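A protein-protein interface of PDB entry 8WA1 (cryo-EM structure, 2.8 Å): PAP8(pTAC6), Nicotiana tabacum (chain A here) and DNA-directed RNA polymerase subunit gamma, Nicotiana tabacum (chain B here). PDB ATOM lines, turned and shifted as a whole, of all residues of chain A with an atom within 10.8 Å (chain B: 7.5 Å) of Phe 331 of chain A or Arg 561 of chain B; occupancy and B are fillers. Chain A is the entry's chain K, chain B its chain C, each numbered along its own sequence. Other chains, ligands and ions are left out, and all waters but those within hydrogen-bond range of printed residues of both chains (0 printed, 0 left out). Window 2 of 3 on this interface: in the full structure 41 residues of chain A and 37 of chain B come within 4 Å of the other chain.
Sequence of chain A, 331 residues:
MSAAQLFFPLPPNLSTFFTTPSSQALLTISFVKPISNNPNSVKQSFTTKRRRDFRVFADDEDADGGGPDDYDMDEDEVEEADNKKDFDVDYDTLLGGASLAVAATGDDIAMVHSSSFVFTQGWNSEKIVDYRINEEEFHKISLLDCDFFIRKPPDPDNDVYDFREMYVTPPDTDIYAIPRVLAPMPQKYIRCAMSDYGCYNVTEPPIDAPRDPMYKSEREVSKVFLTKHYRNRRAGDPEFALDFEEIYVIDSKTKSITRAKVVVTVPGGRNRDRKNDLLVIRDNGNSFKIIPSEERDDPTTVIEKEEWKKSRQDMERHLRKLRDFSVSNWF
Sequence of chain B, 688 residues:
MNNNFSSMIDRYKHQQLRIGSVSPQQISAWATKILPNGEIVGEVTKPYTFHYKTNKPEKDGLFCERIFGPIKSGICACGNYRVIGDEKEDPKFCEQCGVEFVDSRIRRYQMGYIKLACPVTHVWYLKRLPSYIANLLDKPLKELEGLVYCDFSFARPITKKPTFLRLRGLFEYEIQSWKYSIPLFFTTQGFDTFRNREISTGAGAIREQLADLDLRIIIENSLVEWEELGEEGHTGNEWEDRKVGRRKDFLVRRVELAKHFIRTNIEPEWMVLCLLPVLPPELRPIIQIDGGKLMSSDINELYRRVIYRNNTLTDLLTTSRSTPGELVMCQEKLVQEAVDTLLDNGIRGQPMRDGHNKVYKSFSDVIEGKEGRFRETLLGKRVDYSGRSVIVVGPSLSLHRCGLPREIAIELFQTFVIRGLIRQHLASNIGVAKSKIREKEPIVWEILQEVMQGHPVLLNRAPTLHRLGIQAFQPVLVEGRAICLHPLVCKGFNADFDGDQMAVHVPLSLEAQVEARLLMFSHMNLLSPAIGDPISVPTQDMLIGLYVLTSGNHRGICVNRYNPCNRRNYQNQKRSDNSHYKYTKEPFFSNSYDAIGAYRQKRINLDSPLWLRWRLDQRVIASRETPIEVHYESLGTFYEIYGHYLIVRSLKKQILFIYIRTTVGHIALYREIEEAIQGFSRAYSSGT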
ATOM      1  N   GLU A 304      16.457 -15.484  -9.397  1.00  0.00           N
ATOM      2  CA  GLU A 304      16.948 -15.987  -8.120  1.00  0.00           C
ATOM      3  C   GLU A 304      16.168 -15.396  -6.956  1.00  0.00           C
ATOM      4  O   GLU A 304      15.905 -16.085  -5.969  1.00  0.00           O
ATOM      5  CB  GLU A 304      18.440 -15.689  -7.975  1.00  0.00           C
ATOM      6  CG  GLU A 304      19.334 -16.527  -8.874  1.00  0.00           C
ATOM      7  CD  GLU A 304      20.800 -16.172  -8.729  1.00  0.00           C
ATOM      8  OE1 GLU A 304      21.111 -15.212  -7.993  1.00  0.00           O
ATOM      9  OE2 GLU A 304      21.644 -16.851  -9.351  1.00  0.00           O
ATOM     10  N   GLU A 307      12.764 -17.244  -6.875  1.00  0.00           N
ATOM     11  CA  GLU A 307      12.994 -18.614  -6.432  1.00  0.00           C
ATOM     12  C   GLU A 307      13.314 -18.667  -4.944  1.00  0.00           C
ATOM     13  O   GLU A 307      12.803 -19.533  -4.225  1.00  0.00           O
ATOM     14  CB  GLU A 307      14.122 -19.249  -7.245  1.00  0.00           C
ATOM     15  CG  GLU A 307      13.726 -19.652  -8.658  1.00  0.00           C
ATOM     16  CD  GLU A 307      12.805 -20.857  -8.685  1.00  0.00           C
ATOM     17  OE1 GLU A 307      12.765 -21.601  -7.681  1.00  0.00           O
ATOM     18  OE2 GLU A 307      12.121 -21.062  -9.709  1.00  0.00           O
ATOM     19  N   TRP A 308      14.149 -17.744  -4.462  1.00  0.00           N
ATOM     20  CA  TRP A 308      14.512 -17.727  -3.051  1.00  0.00           C
ATOM     21  C   TRP A 308      13.306 -17.414  -2.178  1.00  0.00           C
ATOM     22  O   TRP A 308      13.124 -18.025  -1.121  1.00  0.00           O
ATOM     23  CB  TRP A 308      15.629 -16.710  -2.816  1.00  0.00           C
ATOM     24  CG  TRP A 308      16.318 -16.852  -1.495  1.00  0.00           C
ATOM     25  CD1 TRP A 308      17.412 -17.621  -1.219  1.00  0.00           C
ATOM     26  CD2 TRP A 308      15.965 -16.203  -0.267  1.00  0.00           C
ATOM     27  NE1 TRP A 308      17.761 -17.492   0.103  1.00  0.00           N
ATOM     28  CE2 TRP A 308      16.888 -16.627   0.709  1.00  0.00           C
ATOM     29  CE3 TRP A 308      14.959 -15.306   0.101  1.00  0.00           C
ATOM     30  CZ2 TRP A 308      16.834 -16.186   2.029  1.00  0.00           C
ATOM     31  CZ3 TRP A 308      14.907 -14.868   1.412  1.00  0.00           C
ATOM     32  CH2 TRP A 308      15.839 -15.308   2.360  1.00  0.00           C
ATOM     33  N   LYS A 309      12.467 -16.469  -2.608  1.00  0.00           N
ATOM     34  CA  LYS A 309      11.267 -16.151  -1.839  1.00  0.00           C
ATOM     35  C   LYS A 309      10.331 -17.352  -1.755  1.00  0.00           C
ATOM     36  O   LYS A 309       9.859 -17.710  -0.665  1.00  0.00           O
ATOM     37  CB  LYS A 309      10.550 -14.951  -2.455  1.00  0.00           C
ATOM     38  CG  LYS A 309       9.252 -14.577  -1.760  1.00  0.00           C
ATOM     39  CD  LYS A 309       8.619 -13.349  -2.394  1.00  0.00           C
ATOM     40  CE  LYS A 309       8.316 -13.578  -3.866  1.00  0.00           C
ATOM     41  NZ  LYS A 309       7.373 -14.712  -4.070  1.00  0.00           N
ATOM     42  N   SER A 311      11.052 -20.511  -2.154  1.00  0.00           N
ATOM     43  CA  SER A 311      11.676 -21.589  -1.397  1.00  0.00           C
ATOM     44  C   SER A 311      11.638 -21.307   0.098  1.00  0.00           C
ATOM     45  O   SER A 311      11.399 -22.216   0.897  1.00  0.00           O
ATOM     46  CB  SER A 311      13.114 -21.795  -1.866  1.00  0.00           C
ATOM     47  OG  SER A 311      13.881 -20.622  -1.667  1.00  0.00           O
ATOM     48  N   ARG A 312      11.869 -20.054   0.496  1.00  0.00           N
ATOM     49  CA  ARG A 312      11.776 -19.700   1.909  1.00  0.00           C
ATOM     50  C   ARG A 312      10.365 -19.919   2.435  1.00  0.00           C
ATOM     51  O   ARG A 312      10.178 -20.488   3.519  1.00  0.00           O
ATOM     52  CB  ARG A 312      12.205 -18.249   2.117  1.00  0.00           C
ATOM     53  CG  ARG A 312      13.587 -18.087   2.723  1.00  0.00           C
ATOM     54  CD  ARG A 312      13.510 -17.454   4.102  1.00  0.00           C
ATOM     55  NE  ARG A 312      12.628 -18.198   4.994  1.00  0.00           N
ATOM     56  CZ  ARG A 312      12.392 -17.863   6.258  1.00  0.00           C
ATOM     57  NH1 ARG A 312      12.975 -16.795   6.783  1.00  0.00           N
ATOM     58  NH2 ARG A 312      11.573 -18.598   6.999  1.00  0.00           N
ATOM     59  N   MET A 315       9.696 -23.683   2.665  1.00  0.00           N
ATOM     60  CA  MET A 315      10.469 -24.317   3.726  1.00  0.00           C
ATOM     61  C   MET A 315       9.900 -23.978   5.096  1.00  0.00           C
ATOM     62  O   MET A 315       9.837 -24.841   5.980  1.00  0.00           O
ATOM     63  CB  MET A 315      11.935 -23.896   3.631  1.00  0.00           C
ATOM     64  CG  MET A 315      12.873 -24.712   4.503  1.00  0.00           C
ATOM     65  SD  MET A 315      12.910 -26.452   4.033  1.00  0.00           S
ATOM     66  CE  MET A 315      14.129 -27.090   5.180  1.00  0.00           C
ATOM     67  N   LEU A 319       8.477 -26.705   7.740  1.00  0.00           N
ATOM     68  CA  LEU A 319       9.047 -26.833   9.075  1.00  0.00           C
ATOM     69  C   LEU A 319       8.103 -26.379  10.180  1.00  0.00           C
ATOM     70  O   LEU A 319       8.388 -26.639  11.353  1.00  0.00           O
ATOM     71  CB  LEU A 319      10.354 -26.043   9.168  1.00  0.00           C
ATOM     72  CG  LEU A 319      11.503 -26.522   8.278  1.00  0.00           C
ATOM     73  CD1 LEU A 319      12.741 -25.668   8.499  1.00  0.00           C
ATOM     74  CD2 LEU A 319      11.806 -27.988   8.537  1.00  0.00           C
ATOM     75  N   ASP A 324       9.111 -28.528  17.377  1.00  0.00           N
ATOM     76  CA  ASP A 324      10.147 -27.633  17.877  1.00  0.00           C
ATOM     77  C   ASP A 324      10.294 -26.379  17.025  1.00  0.00           C
ATOM     78  O   ASP A 324      11.315 -25.691  17.124  1.00  0.00           O
ATOM     79  CB  ASP A 324      11.485 -28.369  17.963  1.00  0.00           C
ATOM     80  CG  ASP A 324      11.477 -29.472  19.001  1.00  0.00           C
ATOM     81  OD1 ASP A 324      10.427 -29.679  19.644  1.00  0.00           O
ATOM     82  OD2 ASP A 324      12.523 -30.132  19.174  1.00  0.00           O
ATOM     83  N   PHE A 325       9.301 -26.071  16.188  1.00  0.00           N
ATOM     84  CA  PHE A 325       9.387 -24.892  15.332  1.00  0.00           C
ATOM     85  C   PHE A 325       9.407 -23.609  16.152  1.00  0.00           C
ATOM     86  O   PHE A 325      10.008 -22.610  15.740  1.00  0.00           O
ATOM     87  CB  PHE A 325       8.223 -24.880  14.342  1.00  0.00           C
ATOM     88  CG  PHE A 325       8.226 -23.700  13.413  1.00  0.00           C
ATOM     89  CD1 PHE A 325       9.054 -23.679  12.303  1.00  0.00           C
ATOM     90  CD2 PHE A 325       7.394 -22.617  13.642  1.00  0.00           C
ATOM     91  CE1 PHE A 325       9.056 -22.598  11.444  1.00  0.00           C
ATOM     92  CE2 PHE A 325       7.392 -21.533  12.787  1.00  0.00           C
ATOM     93  CZ  PHE A 325       8.226 -21.523  11.686  1.00  0.00           C
ATOM     94  N   VAL A 327      10.766 -22.913  19.313  1.00  0.00           N
ATOM     95  CA  VAL A 327      12.135 -22.643  19.790  1.00  0.00           C
ATOM     96  C   VAL A 327      13.069 -23.122  18.684  1.00  0.00           C
ATOM     97  O   VAL A 327      13.564 -24.252  18.672  1.00  0.00           O
ATOM     98  CB  VAL A 327      12.417 -23.301  21.144  1.00  0.00           C
ATOM     99  CG1 VAL A 327      11.924 -22.412  22.273  1.00  0.00           C
ATOM    100  CG2 VAL A 327      11.743 -24.663  21.223  1.00  0.00           C
ATOM    101  N   SER A 328      13.317 -22.234  17.725  1.00  0.00           N
ATOM    102  CA  SER A 328      14.174 -22.541  16.590  1.00  0.00           C
ATOM    103  C   SER A 328      14.756 -21.245  16.047  1.00  0.00           C
ATOM    104  O   SER A 328      14.372 -20.146  16.456  1.00  0.00           O
ATOM    105  CB  SER A 328      13.409 -23.296  15.498  1.00  0.00           C
ATOM    106  OG  SER A 328      12.974 -24.563  15.957  1.00  0.00           O
ATOM    107  N   ASN A 329      15.693 -21.386  15.113  1.00  0.00           N
ATOM    108  CA  ASN A 329      16.357 -20.236  14.513  1.00  0.00           C
ATOM    109  C   ASN A 329      16.703 -20.569  13.071  1.00  0.00           C
ATOM    110  O   ASN A 329      17.343 -21.591  12.806  1.00  0.00           O
ATOM    111  CB  ASN A 329      17.619 -19.859  15.298  1.00  0.00           C
ATOM    112  CG  ASN A 329      18.157 -18.491  14.924  1.00  0.00           C
ATOM    113  OD1 ASN A 329      18.253 -18.145  13.748  1.00  0.00           O
ATOM    114  ND2 ASN A 329      18.508 -17.702  15.933  1.00  0.00           N
ATOM    115  N   TRP A 330      16.279 -19.710  12.147  1.00  0.00           N
ATOM    116  CA  TRP A 330      16.599 -19.896  10.739  1.00  0.00           C
ATOM    117  C   TRP A 330      17.987 -19.342  10.451  1.00  0.00           C
ATOM    118  O   TRP A 330      18.217 -18.135  10.564  1.00  0.00           O
ATOM    119  CB  TRP A 330      15.561 -19.209   9.853  1.00  0.00           C
ATOM    120  CG  TRP A 330      15.661 -19.592   8.404  1.00  0.00           C
ATOM    121  CD1 TRP A 330      14.968 -20.582   7.769  1.00  0.00           C
ATOM    122  CD2 TRP A 330      16.503 -18.993   7.412  1.00  0.00           C
ATOM    123  NE1 TRP A 330      15.326 -20.637   6.445  1.00  0.00           N
ATOM    124  CE2 TRP A 330      16.267 -19.672   6.200  1.00  0.00           C
ATOM    125  CE3 TRP A 330      17.433 -17.950   7.430  1.00  0.00           C
ATOM    126  CZ2 TRP A 330      16.927 -19.342   5.019  1.00  0.00           C
ATOM    127  CZ3 TRP A 330      18.087 -17.625   6.258  1.00  0.00           C
ATOM    128  CH2 TRP A 330      17.830 -18.317   5.068  1.00  0.00           C
ATOM    129  N   PHE A 331      18.908 -20.223  10.076  1.00  0.00           N
ATOM    130  CA  PHE A 331      20.282 -19.821   9.807  1.00  0.00           C
ATOM    131  C   PHE A 331      20.645 -20.058   8.346  1.00  0.00           C
ATOM    132  O   PHE A 331      21.589 -19.466   7.824  1.00  0.00           O
ATOM    133  CB  PHE A 331      21.249 -20.576  10.724  1.00  0.00           C
ATOM    134  CG  PHE A 331      21.102 -22.069  10.662  1.00  0.00           C
ATOM    135  CD1 PHE A 331      20.223 -22.728  11.505  1.00  0.00           C
ATOM    136  CD2 PHE A 331      21.845 -22.816   9.763  1.00  0.00           C
ATOM    137  CE1 PHE A 331      20.085 -24.099  11.450  1.00  0.00           C
ATOM    138  CE2 PHE A 331      21.711 -24.188   9.704  1.00  0.00           C
ATOM    139  CZ  PHE A 331      20.830 -24.830  10.549  1.00  0.00           C
ATOM    140  OXT PHE A 331      20.003 -20.849   7.655  1.00  0.00           O
ATOM    141  N   GLY B 556      16.380 -22.324  -4.908  1.00  0.00           N
ATOM    142  CA  GLY B 556      16.030 -21.334  -3.908  1.00  0.00           C
ATOM    143  C   GLY B 556      17.056 -21.120  -2.817  1.00  0.00           C
ATOM    144  O   GLY B 556      18.143 -20.593  -3.067  1.00  0.00           O
ATOM    145  N   ILE B 557      16.716 -21.522  -1.591  1.00  0.00           N
ATOM    146  CA  ILE B 557      17.592 -21.258  -0.451  1.00  0.00           C
ATOM    147  C   ILE B 557      18.830 -22.140  -0.509  1.00  0.00           C
ATOM    148  O   ILE B 557      19.839 -21.860   0.147  1.00  0.00           O
ATOM    149  CB  ILE B 557      16.821 -21.453   0.867  1.00  0.00           C
ATOM    150  CG1 ILE B 557      16.231 -22.861   0.932  1.00  0.00           C
ATOM    151  CG2 ILE B 557      15.736 -20.404   1.004  1.00  0.00           C
ATOM    152  CD1 ILE B 557      15.400 -23.114   2.165  1.00  0.00           C
ATOM    153  N   CYS B 558      18.772 -23.223  -1.286  1.00  0.00           N
ATOM    154  CA  CYS B 558      19.897 -24.147  -1.346  1.00  0.00           C
ATOM    155  C   CYS B 558      21.070 -23.548  -2.114  1.00  0.00           C
ATOM    156  O   CYS B 558      22.231 -23.861  -1.828  1.00  0.00           O
ATOM    157  CB  CYS B 558      19.455 -25.465  -1.980  1.00  0.00           C
ATOM    158  SG  CYS B 558      18.092 -26.284  -1.122  1.00  0.00           S
ATOM    159  N   VAL B 559      20.788 -22.685  -3.093  1.00  0.00           N
ATOM    160  CA  VAL B 559      21.853 -22.171  -3.948  1.00  0.00           C
ATOM    161  C   VAL B 559      22.462 -20.902  -3.358  1.00  0.00           C
ATOM    162  O   VAL B 559      23.637 -20.595  -3.598  1.00  0.00           O
ATOM    163  CB  VAL B 559      21.323 -21.939  -5.376  1.00  0.00           C
ATOM    164  CG1 VAL B 559      20.333 -20.783  -5.411  1.00  0.00           C
ATOM    165  CG2 VAL B 559      22.472 -21.705  -6.347  1.00  0.00           C
ATOM    166  N   ASN B 560      21.690 -20.150  -2.576  1.00  0.00           N
ATOM    167  CA  ASN B 560      22.144 -18.885  -2.014  1.00  0.00           C
ATOM    168  C   ASN B 560      21.814 -18.827  -0.531  1.00  0.00           C
ATOM    169  O   ASN B 560      20.733 -19.249  -0.111  1.00  0.00           O
ATOM    170  CB  ASN B 560      21.504 -17.693  -2.736  1.00  0.00           C
ATOM    171  CG  ASN B 560      21.893 -17.618  -4.196  1.00  0.00           C
ATOM    172  OD1 ASN B 560      23.011 -17.973  -4.572  1.00  0.00           O
ATOM    173  ND2 ASN B 560      20.972 -17.152  -5.031  1.00  0.00           N
ATOM    174  N   ARG B 561      22.747 -18.293   0.258  1.00  0.00           N
ATOM    175  CA  ARG B 561      22.525 -18.173   1.692  1.00  0.00           C
ATOM    176  C   ARG B 561      21.735 -16.926   2.065  1.00  0.00           C
ATOM    177  O   ARG B 561      20.951 -16.966   3.019  1.00  0.00           O
ATOM    178  CB  ARG B 561      23.859 -18.171   2.440  1.00  0.00           C
ATOM    179  CG  ARG B 561      23.705 -18.219   3.950  1.00  0.00           C
ATOM    180  CD  ARG B 561      25.021 -17.999   4.663  1.00  0.00           C
ATOM    181  NE  ARG B 561      24.846 -17.973   6.110  1.00  0.00           N
ATOM    182  CZ  ARG B 561      25.830 -17.773   6.980  1.00  0.00           C
ATOM    183  NH1 ARG B 561      25.577 -17.766   8.281  1.00  0.00           N
ATOM    184  NH2 ARG B 561      27.070 -17.580   6.549  1.00  0.00           N
ATOM    185  N   TYR B 562      21.904 -15.833   1.325  1.00  0.00           N
ATOM    186  CA  TYR B 562      21.197 -14.593   1.603  1.00  0.00           C
ATOM    187  C   TYR B 562      20.306 -14.259   0.417  1.00  0.00           C
ATOM    188  O   TYR B 562      20.501 -14.760  -0.693  1.00  0.00           O
ATOM    189  CB  TYR B 562      22.164 -13.436   1.887  1.00  0.00           C
ATOM    190  CG  TYR B 562      23.120 -13.701   3.028  1.00  0.00           C
ATOM    191  CD1 TYR B 562      22.753 -13.446   4.341  1.00  0.00           C
ATOM    192  CD2 TYR B 562      24.392 -14.205   2.789  1.00  0.00           C
ATOM    193  CE1 TYR B 562      23.624 -13.687   5.387  1.00  0.00           C
ATOM    194  CE2 TYR B 562      25.269 -14.449   3.828  1.00  0.00           C
ATOM    195  CZ  TYR B 562      24.880 -14.188   5.124  1.00  0.00           C
ATOM    196  OH  TYR B 562      25.750 -14.428   6.163  1.00  0.00           O
ATOM    197  N   ASN B 563      19.321 -13.407   0.671  1.00  0.00           N
ATOM    198  CA  ASN B 563      18.396 -13.011  -0.379  1.00  0.00           C
ATOM    199  C   ASN B 563      19.137 -12.205  -1.444  1.00  0.00           C
ATOM    200  O   ASN B 563      19.849 -11.248  -1.116  1.00  0.00           O
ATOM    201  CB  ASN B 563      17.252 -12.184   0.212  1.00  0.00           C
ATOM    202  CG  ASN B 563      16.067 -12.051  -0.731  1.00  0.00           C
ATOM    203  OD1 ASN B 563      16.227 -11.931  -1.945  1.00  0.00           O
ATOM    204  ND2 ASN B 563      14.865 -12.065  -0.167  1.00  0.00           N
ATOM    205  N   PRO B 564      19.001 -12.564  -2.725  1.00  0.00           N
ATOM    206  CA  PRO B 564      19.643 -11.771  -3.786  1.00  0.00           C
ATOM    207  C   PRO B 564      19.079 -10.367  -3.938  1.00  0.00           C
ATOM    208  O   PRO B 564      19.549  -9.629  -4.815  1.00  0.00           O
ATOM    209  CB  PRO B 564      19.390 -12.605  -5.051  1.00  0.00           C
ATOM    210  CG  PRO B 564      19.134 -13.992  -4.549  1.00  0.00           C
ATOM    211  CD  PRO B 564      18.424 -13.816  -3.243  1.00  0.00           C
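The indole nitrogen of Trp 308 of chain A is in hydrogen-bond range of the backbone carbonyl oxygen of Asn 560 of chain B (3.5 Å).
O of Phe 331 of chain A is in salt-bridge range of NE of Arg 561 of chain B (3.97 Å).
The side-chain hydroxyl (OG) of Ser 311 of chain A lies within hydrogen-bond range of the backbone NH (N) of Ile 557 of chain B, at 3.0 Å.
The guanidinium group (NH2) of Arg 561 of chain B is in hydrogen-bond range of the side-chain hydroxyl (OH) of Tyr 562 of chain B (3.4 Å).
O of Trp 308 of chain A lies within hydrogen-bond range of OG of Ser 311 of chain A, 2.8 Å away.
The backbone carbonyl oxygen of Glu 307 of chain A sits at hydrogen-bond distance from the side-chain hydroxyl of Ser 311 of chain A.
Among the printed residues, pairs that only touch across the chains: Glu 304 of chain A with Asn 560 of chain B, Glu 304 of chain A with Pro 564 of chain B, Glu 307 of chain A with Gly 556 of chain B, Trp 308 of chain A with Gly 556 of chain B, Trp 308 of chain A with Ile 557 of chain B, Trp 308 of chain A with Tyr 562 of chain B, Trp 308 of chain A with Asn 563 of chain B, Ser 311 of chain A with Gly 556 of chain B, Arg 312 of chain A with Ile 557 of chain B, Met 315 of chain A with Ile 557 of chain B and Trp 330 of chain A with Arg 561 of chain B.
Of the printed residues of chain B, Glu 307 of chain A touches Gly 556 (3.7 Å).
Printed residues of chain B within 4 Å of Trp 308 of chain A: Gly 556, Ile 557, Asn 560, Tyr 562 and Asn 563.
Printed residues of chain B within 4 Å of Trp 330 of chain A: Arg 561.
Of chain A, only Glu 304 (3.5 Å) and Trp 308 (3.5 Å) come within 4 Å of Asn 560 of chain B.
Of chain A, only Trp 330 and Phe 331 come within 4 Å of Arg 561 of chain B.
Of the printed residues of chain A, Tyr 562 of chain B touches Trp 308 (3.95 Å).
Printed residues of chain A within 4 Å of Asn 563 of chain B: Trp 308.
Of the printed residues of chain A, Pro 564 of chain B touches Glu 304 (3.9 Å).
The nearest residue of chain A that does not touch Arg 561 of chain B is Trp 308 of chain A (4.3 Å).
Hydrophobic or aromatic side chains of chain A that line the printed part of chain B: Trp 308, Met 315 and Trp 330.
Among the printed residues, 14 pairs touch across the chains.
Among the printed residues, no Asp or Glu carboxylate lies within 4 Å of a Lys or Arg side-chain nitrogen of the other chain.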
